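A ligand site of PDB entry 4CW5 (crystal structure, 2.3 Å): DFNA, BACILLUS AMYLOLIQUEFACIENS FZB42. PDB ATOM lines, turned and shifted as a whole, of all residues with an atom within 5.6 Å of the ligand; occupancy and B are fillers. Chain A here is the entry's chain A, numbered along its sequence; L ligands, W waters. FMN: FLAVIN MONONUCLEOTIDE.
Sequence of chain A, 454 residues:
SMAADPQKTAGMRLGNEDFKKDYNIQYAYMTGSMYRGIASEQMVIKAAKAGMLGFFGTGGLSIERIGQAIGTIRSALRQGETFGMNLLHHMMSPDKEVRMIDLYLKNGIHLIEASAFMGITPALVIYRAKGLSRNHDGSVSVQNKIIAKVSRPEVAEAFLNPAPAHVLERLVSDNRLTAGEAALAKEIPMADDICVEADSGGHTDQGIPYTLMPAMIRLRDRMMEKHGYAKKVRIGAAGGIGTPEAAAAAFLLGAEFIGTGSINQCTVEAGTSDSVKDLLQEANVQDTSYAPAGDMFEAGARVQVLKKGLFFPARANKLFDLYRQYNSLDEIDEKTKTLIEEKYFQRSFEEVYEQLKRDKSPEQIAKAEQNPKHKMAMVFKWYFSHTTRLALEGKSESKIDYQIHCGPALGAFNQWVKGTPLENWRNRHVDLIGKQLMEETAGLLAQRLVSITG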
ATOM      1  N   GLY A  32      28.594   9.740 -11.921  1.00  0.00           N
ATOM      2  CA  GLY A  32      29.448  10.167 -10.837  1.00  0.00           C
ATOM      3  C   GLY A  32      29.025   9.595  -9.500  1.00  0.00           C
ATOM      4  O   GLY A  32      27.876   9.217  -9.312  1.00  0.00           O
ATOM      5  N   SER A  33      29.978   9.510  -8.582  1.00  0.00           N
ATOM      6  CA  SER A  33      29.702   9.029  -7.233  1.00  0.00           C
ATOM      7  C   SER A  33      28.670   9.918  -6.556  1.00  0.00           C
ATOM      8  O   SER A  33      28.613  11.133  -6.809  1.00  0.00           O
ATOM      9  CB  SER A  33      30.979   8.992  -6.401  1.00  0.00           C
ATOM     10  OG  SER A  33      31.960   8.191  -7.038  1.00  0.00           O
ATOM     11  N   MET A  34      27.863   9.318  -5.691  1.00  0.00           N
ATOM     12  CA  MET A  34      26.905  10.068  -4.883  1.00  0.00           C
ATOM     13  C   MET A  34      26.889   9.484  -3.484  1.00  0.00           C
ATOM     14  O   MET A  34      26.536   8.328  -3.290  1.00  0.00           O
ATOM     15  CB  MET A  34      25.518  10.044  -5.523  1.00  0.00           C
ATOM     16  CG  MET A  34      25.495  10.754  -6.876  1.00  0.00           C
ATOM     17  SD  MET A  34      23.735  10.919  -7.669  1.00  0.00           S
ATOM     18  CE  MET A  34      23.316   9.030  -7.925  1.00  0.00           C
ATOM     19  N   TYR A  35      27.278  10.319  -2.504  1.00  0.00           N
ATOM     20  CA  TYR A  35      27.646   9.851  -1.168  1.00  0.00           C
ATOM     21  C   TYR A  35      26.575   9.013  -0.470  1.00  0.00           C
ATOM     22  O   TYR A  35      25.414   8.990  -0.881  1.00  0.00           O
ATOM     23  CB  TYR A  35      27.985  11.044  -0.268  1.00  0.00           C
ATOM     24  CG  TYR A  35      26.862  12.036  -0.090  1.00  0.00           C
ATOM     25  CD1 TYR A  35      25.725  11.691   0.634  1.00  0.00           C
ATOM     26  CD2 TYR A  35      26.928  13.315  -0.620  1.00  0.00           C
ATOM     27  CE1 TYR A  35      24.692  12.571   0.810  1.00  0.00           C
ATOM     28  CE2 TYR A  35      25.899  14.214  -0.455  1.00  0.00           C
ATOM     29  CZ  TYR A  35      24.783  13.832   0.270  1.00  0.00           C
ATOM     30  OH  TYR A  35      23.731  14.694   0.461  1.00  0.00           O
ATOM     31  N   ILE A  38      23.976   6.723  -2.289  1.00  0.00           N
ATOM     32  CA  ILE A  38      22.956   7.234  -3.205  1.00  0.00           C
ATOM     33  C   ILE A  38      23.290   6.729  -4.600  1.00  0.00           C
ATOM     34  O   ILE A  38      22.404   6.316  -5.353  1.00  0.00           O
ATOM     35  CB  ILE A  38      22.865   8.768  -3.185  1.00  0.00           C
ATOM     36  CG1 ILE A  38      22.416   9.255  -1.807  1.00  0.00           C
ATOM     37  CG2 ILE A  38      21.882   9.259  -4.254  1.00  0.00           C
ATOM     38  CD1 ILE A  38      22.492  10.753  -1.607  1.00  0.00           C
ATOM     39  N   GLY A  59      31.218   7.828   0.055  1.00  0.00           N
ATOM     40  CA  GLY A  59      31.216   8.967   0.955  1.00  0.00           C
ATOM     41  C   GLY A  59      30.375   8.773   2.205  1.00  0.00           C
ATOM     42  O   GLY A  59      29.168   8.577   2.132  1.00  0.00           O
ATOM     43  N   ASN A  86      34.220   5.450  -5.366  1.00  0.00           N
ATOM     44  CA  ASN A  86      34.615   6.802  -5.001  1.00  0.00           C
ATOM     45  C   ASN A  86      35.727   6.772  -3.968  1.00  0.00           C
ATOM     46  O   ASN A  86      35.673   5.974  -3.035  1.00  0.00           O
ATOM     47  CB  ASN A  86      33.427   7.590  -4.441  1.00  0.00           C
ATOM     48  CG  ASN A  86      33.659   9.103  -4.419  1.00  0.00           C
ATOM     49  OD1 ASN A  86      33.041   9.816  -3.629  1.00  0.00           O
ATOM     50  ND2 ASN A  86      34.524   9.613  -5.301  1.00  0.00           N
ATOM     51  N   LEU A  88      36.831   9.782  -1.780  1.00  0.00           N
ATOM     52  CA  LEU A  88      36.558  11.178  -1.469  1.00  0.00           C
ATOM     53  C   LEU A  88      37.533  11.664  -0.414  1.00  0.00           C
ATOM     54  O   LEU A  88      37.583  11.128   0.692  1.00  0.00           O
ATOM     55  CB  LEU A  88      35.116  11.338  -1.003  1.00  0.00           C
ATOM     56  CG  LEU A  88      34.568  12.752  -0.837  1.00  0.00           C
ATOM     57  CD1 LEU A  88      34.618  13.521  -2.149  1.00  0.00           C
ATOM     58  CD2 LEU A  88      33.150  12.685  -0.299  1.00  0.00           C
ATOM     59  N   GLU A 113      37.164   6.751  -8.580  1.00  0.00           N
ATOM     60  CA  GLU A 113      36.986   8.156  -8.876  1.00  0.00           C
ATOM     61  C   GLU A 113      37.558   8.940  -7.705  1.00  0.00           C
ATOM     62  O   GLU A 113      37.028   8.890  -6.601  1.00  0.00           O
ATOM     63  CB  GLU A 113      35.500   8.502  -9.093  1.00  0.00           C
ATOM     64  CG  GLU A 113      35.233   9.996  -9.197  1.00  0.00           C
ATOM     65  CD  GLU A 113      33.755  10.308  -9.379  1.00  0.00           C
ATOM     66  OE1 GLU A 113      32.901   9.542  -8.888  1.00  0.00           O
ATOM     67  OE2 GLU A 113      33.451  11.349 -10.008  1.00  0.00           O
ATOM     68  N   SER A 115      38.237  12.349  -5.920  1.00  0.00           N
ATOM     69  CA  SER A 115      37.659  13.689  -5.901  1.00  0.00           C
ATOM     70  C   SER A 115      37.995  14.475  -4.631  1.00  0.00           C
ATOM     71  O   SER A 115      38.394  13.904  -3.613  1.00  0.00           O
ATOM     72  CB  SER A 115      36.145  13.600  -6.066  1.00  0.00           C
ATOM     73  OG  SER A 115      35.607  12.581  -5.245  1.00  0.00           O
ATOM     74  N   ALA A 116      37.838  15.796  -4.730  1.00  0.00           N
ATOM     75  CA  ALA A 116      38.109  16.732  -3.639  1.00  0.00           C
ATOM     76  C   ALA A 116      39.560  16.735  -3.161  1.00  0.00           C
ATOM     77  O   ALA A 116      39.872  17.318  -2.123  1.00  0.00           O
ATOM     78  CB  ALA A 116      37.184  16.430  -2.459  1.00  0.00           C
ATOM     79  N   LYS A 149      38.629  13.647 -10.550  1.00  0.00           N
ATOM     80  CA  LYS A 149      37.618  14.684 -10.764  1.00  0.00           C
ATOM     81  C   LYS A 149      38.101  15.963 -10.096  1.00  0.00           C
ATOM     82  O   LYS A 149      38.299  16.002  -8.879  1.00  0.00           O
ATOM     83  CB  LYS A 149      36.260  14.254 -10.209  1.00  0.00           C
ATOM     84  CG  LYS A 149      35.147  15.200 -10.614  1.00  0.00           C
ATOM     85  CD  LYS A 149      33.771  14.579 -10.437  1.00  0.00           C
ATOM     86  CE  LYS A 149      33.487  14.188  -9.001  1.00  0.00           C
ATOM     87  NZ  LYS A 149      32.166  13.522  -8.879  1.00  0.00           N
ATOM     88  N   GLU A 197      35.274  19.310 -13.627  1.00  0.00           N
ATOM     89  CA  GLU A 197      33.957  19.578 -13.073  1.00  0.00           C
ATOM     90  C   GLU A 197      33.651  21.071 -13.055  1.00  0.00           C
ATOM     91  O   GLU A 197      34.420  21.871 -12.522  1.00  0.00           O
ATOM     92  CB  GLU A 197      33.839  19.002 -11.671  1.00  0.00           C
ATOM     93  CG  GLU A 197      32.406  18.982 -11.169  1.00  0.00           C
ATOM     94  CD  GLU A 197      32.238  18.202  -9.881  1.00  0.00           C
ATOM     95  OE1 GLU A 197      33.237  18.070  -9.131  1.00  0.00           O
ATOM     96  OE2 GLU A 197      31.119  17.714  -9.623  1.00  0.00           O
ATOM     97  N   ALA A 238      32.163  17.211 -16.621  1.00  0.00           N
ATOM     98  CA  ALA A 238      30.975  16.970 -15.812  1.00  0.00           C
ATOM     99  C   ALA A 238      30.482  18.266 -15.195  1.00  0.00           C
ATOM    100  O   ALA A 238      31.261  19.201 -15.012  1.00  0.00           O
ATOM    101  CB  ALA A 238      31.256  15.929 -14.740  1.00  0.00           C
ATOM    102  N   GLY A 239      29.190  18.331 -14.912  1.00  0.00           N
ATOM    103  CA  GLY A 239      28.591  19.524 -14.340  1.00  0.00           C
ATOM    104  C   GLY A 239      27.677  20.221 -15.326  1.00  0.00           C
ATOM    105  O   GLY A 239      28.124  20.674 -16.375  1.00  0.00           O
ATOM    106  N   GLY A 240      26.402  20.307 -14.985  1.00  0.00           N
ATOM    107  CA  GLY A 240      25.430  21.019 -15.816  1.00  0.00           C
ATOM    108  C   GLY A 240      24.895  20.207 -16.979  1.00  0.00           C
ATOM    109  O   GLY A 240      24.133  20.730 -17.789  1.00  0.00           O
ATOM    110  N   ILE A 241      25.276  18.931 -17.059  1.00  0.00           N
ATOM    111  CA  ILE A 241      24.894  18.109 -18.197  1.00  0.00           C
ATOM    112  C   ILE A 241      23.687  17.243 -17.846  1.00  0.00           C
ATOM    113  O   ILE A 241      23.787  16.314 -17.046  1.00  0.00           O
ATOM    114  CB  ILE A 241      26.047  17.216 -18.681  1.00  0.00           C
ATOM    115  CG1 ILE A 241      27.269  18.075 -19.029  1.00  0.00           C
ATOM    116  CG2 ILE A 241      25.616  16.396 -19.891  1.00  0.00           C
ATOM    117  CD1 ILE A 241      28.509  17.271 -19.349  1.00  0.00           C
ATOM    118  N   GLY A 259      30.545  12.966 -17.709  1.00  0.00           N
ATOM    119  CA  GLY A 259      29.971  12.382 -16.516  1.00  0.00           C
ATOM    120  C   GLY A 259      28.702  13.116 -16.130  1.00  0.00           C
ATOM    121  O   GLY A 259      28.589  14.316 -16.370  1.00  0.00           O
ATOM    122  N   THR A 260      27.755  12.382 -15.558  1.00  0.00           N
ATOM    123  CA  THR A 260      26.513  12.983 -15.053  1.00  0.00           C
ATOM    124  C   THR A 260      26.347  12.635 -13.574  1.00  0.00           C
ATOM    125  O   THR A 260      26.901  11.654 -13.086  1.00  0.00           O
ATOM    126  CB  THR A 260      25.288  12.483 -15.823  1.00  0.00           C
ATOM    127  OG1 THR A 260      25.225  11.052 -15.778  1.00  0.00           O
ATOM    128  CG2 THR A 260      25.330  12.941 -17.265  1.00  0.00           C
ATOM    129  N   GLY A 261      25.549  13.445 -12.888  1.00  0.00           N
ATOM    130  CA  GLY A 261      25.280  13.231 -11.481  1.00  0.00           C
ATOM    131  C   GLY A 261      23.817  13.447 -11.125  1.00  0.00           C
ATOM    132  O   GLY A 261      23.098  12.497 -10.801  1.00  0.00           O
ATOM    133  N   SER A 262      23.388  14.697 -11.186  1.00  0.00           N
ATOM    134  CA  SER A 262      22.068  15.105 -10.722  1.00  0.00           C
ATOM    135  C   SER A 262      20.932  14.274 -11.326  1.00  0.00           C
ATOM    136  O   SER A 262      20.008  13.884 -10.624  1.00  0.00           O
ATOM    137  CB  SER A 262      21.828  16.587 -11.040  1.00  0.00           C
ATOM    138  OG  SER A 262      22.548  17.410 -10.136  1.00  0.00           O
ATOM    139  N   ILE A 263      21.002  14.007 -12.627  1.00  0.00           N
ATOM    140  CA  ILE A 263      19.920  13.284 -13.294  1.00  0.00           C
ATOM    141  C   ILE A 263      19.800  11.853 -12.771  1.00  0.00           C
ATOM    142  O   ILE A 263      18.728  11.261 -12.849  1.00  0.00           O
ATOM    143  CB  ILE A 263      20.118  13.257 -14.831  1.00  0.00           C
ATOM    144  CG1 ILE A 263      21.379  12.471 -15.210  1.00  0.00           C
ATOM    145  CG2 ILE A 263      20.171  14.674 -15.380  1.00  0.00           C
ATOM    146  CD1 ILE A 263      21.599  12.320 -16.702  1.00  0.00           C
ATOM    147  N   GLN A 265      20.281  10.823  -9.581  1.00  0.00           N
ATOM    148  CA  GLN A 265      19.678  10.733  -8.258  1.00  0.00           C
ATOM    149  C   GLN A 265      18.183  10.510  -8.388  1.00  0.00           C
ATOM    150  O   GLN A 265      17.551   9.928  -7.504  1.00  0.00           O
ATOM    151  CB  GLN A 265      19.954  12.000  -7.441  1.00  0.00           C
ATOM    152  CG  GLN A 265      19.561  11.858  -5.964  1.00  0.00           C
ATOM    153  CD  GLN A 265      19.938  13.077  -5.118  1.00  0.00           C
ATOM    154  OE1 GLN A 265      20.236  12.937  -3.929  1.00  0.00           O
ATOM    155  NE2 GLN A 265      19.905  14.256  -5.720  1.00  0.00           N
ATOM    156  N   HIS A 405      21.241  17.361  -2.411  1.00  0.00           N
ATOM    157  CA  HIS A 405      22.202  17.922  -3.350  1.00  0.00           C
ATOM    158  C   HIS A 405      21.677  17.729  -4.764  1.00  0.00           C
ATOM    159  O   HIS A 405      21.223  16.644  -5.125  1.00  0.00           O
ATOM    160  CB  HIS A 405      23.570  17.271  -3.187  1.00  0.00           C
ATOM    161  CG  HIS A 405      24.233  17.594  -1.877  1.00  0.00           C
ATOM    162  ND1 HIS A 405      23.914  16.934  -0.705  1.00  0.00           N
ATOM    163  CD2 HIS A 405      25.202  18.479  -1.562  1.00  0.00           C
ATOM    164  CE1 HIS A 405      24.656  17.424   0.282  1.00  0.00           C
ATOM    165  NE2 HIS A 405      25.442  18.354  -0.218  1.00  0.00           N
ATOM    166  N   CYS A 406      21.776  18.787  -5.557  1.00  0.00           N
ATOM    167  CA  CYS A 406      21.161  18.807  -6.886  1.00  0.00           C
ATOM    168  C   CYS A 406      21.543  20.092  -7.626  1.00  0.00           C
ATOM    169  O   CYS A 406      21.600  21.152  -7.026  1.00  0.00           O
ATOM    170  CB  CYS A 406      19.637  18.701  -6.769  1.00  0.00           C
ATOM    171  SG  CYS A 406      18.777  18.507  -8.331  1.00  0.00           S
ATOM    172  N   GLY A 407      21.773  19.964  -8.930  1.00  0.00           N
ATOM    173  CA  GLY A 407      22.092  21.102  -9.767  1.00  0.00           C
ATOM    174  C   GLY A 407      21.012  21.313 -10.817  1.00  0.00           C
ATOM    175  O   GLY A 407      20.119  20.486 -10.952  1.00  0.00           O
ATOM    176  N   ALA A 409      21.051  20.871 -13.871  1.00  0.00           N
ATOM    177  CA  ALA A 409      21.041  19.810 -14.876  1.00  0.00           C
ATOM    178  C   ALA A 409      19.769  18.976 -14.789  1.00  0.00           C
ATOM    179  O   ALA A 409      19.197  18.612 -15.821  1.00  0.00           O
ATOM    180  CB  ALA A 409      22.259  18.920 -14.711  1.00  0.00           C
HETATM  181  N1  FMN L   1      30.947  13.703  -6.053  1.00  0.00           N
HETATM  182  C2  FMN L   1      31.952  13.136  -5.286  1.00  0.00           C
HETATM  183  O2  FMN L   1      33.115  13.195  -5.687  1.00  0.00           O
HETATM  184  N3  FMN L   1      31.654  12.513  -4.098  1.00  0.00           N
HETATM  185  C4  FMN L   1      30.346  12.463  -3.669  1.00  0.00           C
HETATM  186  O4  FMN L   1      30.074  11.906  -2.606  1.00  0.00           O
HETATM  187  C4A FMN L   1      29.327  13.030  -4.431  1.00  0.00           C
HETATM  188  N5  FMN L   1      28.021  12.973  -3.996  1.00  0.00           N
HETATM  189  C5A FMN L   1      27.024  13.545  -4.759  1.00  0.00           C
HETATM  190  C6  FMN L   1      25.706  13.472  -4.335  1.00  0.00           C
HETATM  191  C7  FMN L   1      24.684  14.039  -5.084  1.00  0.00           C
HETATM  192  C7M FMN L   1      23.279  13.922  -4.570  1.00  0.00           C
HETATM  193  C8  FMN L   1      24.999  14.662  -6.290  1.00  0.00           C
HETATM  194  C8M FMN L   1      23.938  15.281  -7.162  1.00  0.00           C
HETATM  195  C9  FMN L   1      26.314  14.724  -6.724  1.00  0.00           C
HETATM  196  C9A FMN L   1      27.331  14.163  -5.968  1.00  0.00           C
HETATM  197  N10 FMN L   1      28.646  14.225  -6.401  1.00  0.00           N
HETATM  198  C10 FMN L   1      29.639  13.652  -5.624  1.00  0.00           C
HETATM  199  C1' FMN L   1      29.003  14.892  -7.702  1.00  0.00           C
HETATM  200  C2' FMN L   1      28.671  13.951  -8.854  1.00  0.00           C
HETATM  201  O2' FMN L   1      29.481  12.797  -8.735  1.00  0.00           O
HETATM  202  C3' FMN L   1      28.901  14.567 -10.230  1.00  0.00           C
HETATM  203  O3' FMN L   1      30.277  14.805 -10.424  1.00  0.00           O
HETATM  204  C4' FMN L   1      28.138  15.875 -10.396  1.00  0.00           C
HETATM  205  O4' FMN L   1      26.866  15.773  -9.801  1.00  0.00           O
HETATM  206  C5' FMN L   1      27.956  16.206 -11.880  1.00  0.00           C
HETATM  207  O5' FMN L   1      27.288  17.442 -11.954  1.00  0.00           O
HETATM  208  P   FMN L   1      25.770  17.522 -12.449  1.00  0.00           P
HETATM  209  O1P FMN L   1      25.486  18.921 -12.963  1.00  0.00           O
HETATM  210  O2P FMN L   1      25.521  16.501 -13.528  1.00  0.00           O
HETATM  211  O3P FMN L   1      24.874  17.212 -11.269  1.00  0.00           O
HETATM  212  O   HOH W   1      21.012  14.432  -2.023  1.00  0.00           O
HETATM  213  O   HOH W   2      30.602   9.249  -2.374  1.00  0.00           O
HETATM  214  O   HOH W   3      23.217  15.354 -14.626  1.00  0.00           O
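N of Ser 262 is in hydrogen-bond range of O3P of the ligand, at 2.9 Å.
OG of Ser 262 is in hydrogen-bond range of O3P of the ligand (2.6 Å).
O2 of the ligand is in hydrogen-bond range of OG of Ser 115 (2.6 Å).
The backbone NH of Gly 240 lies within hydrogen-bond range of an oxygen (O1P) of the ligand (2.6 Å).
The backbone NH of Ser 33 sits at hydrogen-bond distance from an oxygen (O2') of the ligand, at 3.3 Å.
The backbone carbonyl oxygen (O) of Ser 33 lies within hydrogen-bond range of an oxygen (O2') of the ligand (2.7 Å).
O3' of the ligand lies within hydrogen-bond range of NZ of Lys 149 (2.8 Å).
The side-chain amide oxygen of Asn 86 lies within hydrogen-bond range of a nitrogen (N3) of the ligand, at 3.1 Å.
The backbone NH of Gly 261 is in hydrogen-bond range of an oxygen (O2P) of the ligand, 3.1 Å away.
The side-chain carboxylate (OE2) of Glu 197 is in hydrogen-bond range of an oxygen (O3') of the ligand (3.1 Å).
N5 of the ligand sits at hydrogen-bond distance from N of Tyr 35, at 3.1 Å.
The side-chain hydroxyl (OG) of Ser 262 is in hydrogen-bond range of the backbone NH (N) of Gly 407.
The side-chain amide nitrogen (ND2) of Asn 86 sits at hydrogen-bond distance from the side-chain hydroxyl (OG) of Ser 115 (3.2 Å).
The side-chain hydroxyl (OG) of Ser 33 sits close to the side-chain amide nitrogen (ND2) of Asn 86 (3.4 Å).
OE1 of Glu 113 is in hydrogen-bond range of OG of Ser 33, 2.5 Å away.
The side-chain carboxylate (OE2) of Glu 113 lies within salt-bridge range of the side-chain amino group (NZ) of Lys 149, 2.8 Å away.
The side-chain amide nitrogen of Asn 86 lies within hydrogen-bond range of the backbone carbonyl oxygen of Glu 113 (2.9 Å).
A ring nitrogen (ND1) of His 405 is in hydrogen-bond range of the side-chain hydroxyl (OH) of Tyr 35 (2.5 Å).
O of His 405 sits at hydrogen-bond distance from NE2 of Gln 265 (2.8 Å).
C of Gly 32 touches O2' of the ligand, 3.3 Å away.
Met 34 touches the ligand.
CD1 of Leu 88 touches N3 of the ligand (3.7 Å).
Gly 239 touches the ligand.
O of Ile 241 touches O2P of the ligand (3.9 Å).
C of Thr 260 touches O2P of the ligand (3.95 Å).
Gln 265 touches the ligand (OE1 to C7M, 3.3 Å).
His 405 touches the ligand (O to C7M, 3.5 Å).
CB of Ala 409 touches O1P of the ligand, at 3.7 Å.
Of the 27 residues printed, 18 come within 4 Å of the ligand.
Water W2 lies within hydrogen-bond range of an oxygen (O4) of the ligand, the side-chain amide oxygen (OD1) of Asn 86, the backbone NH (N) of Gly 59 and the backbone NH (N) of Tyr 35.
Water W3 lies within hydrogen-bond range of the backbone carbonyl oxygen of Ile 241 (2.7 Å), an oxygen (O2P) of the ligand (2.8 Å), the backbone NH of Ile 263 (3.3 Å) and the backbone NH of Gly 261 (3.5 Å).
Water W1 bridges OE1 of Gln 265 and N of His 405.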
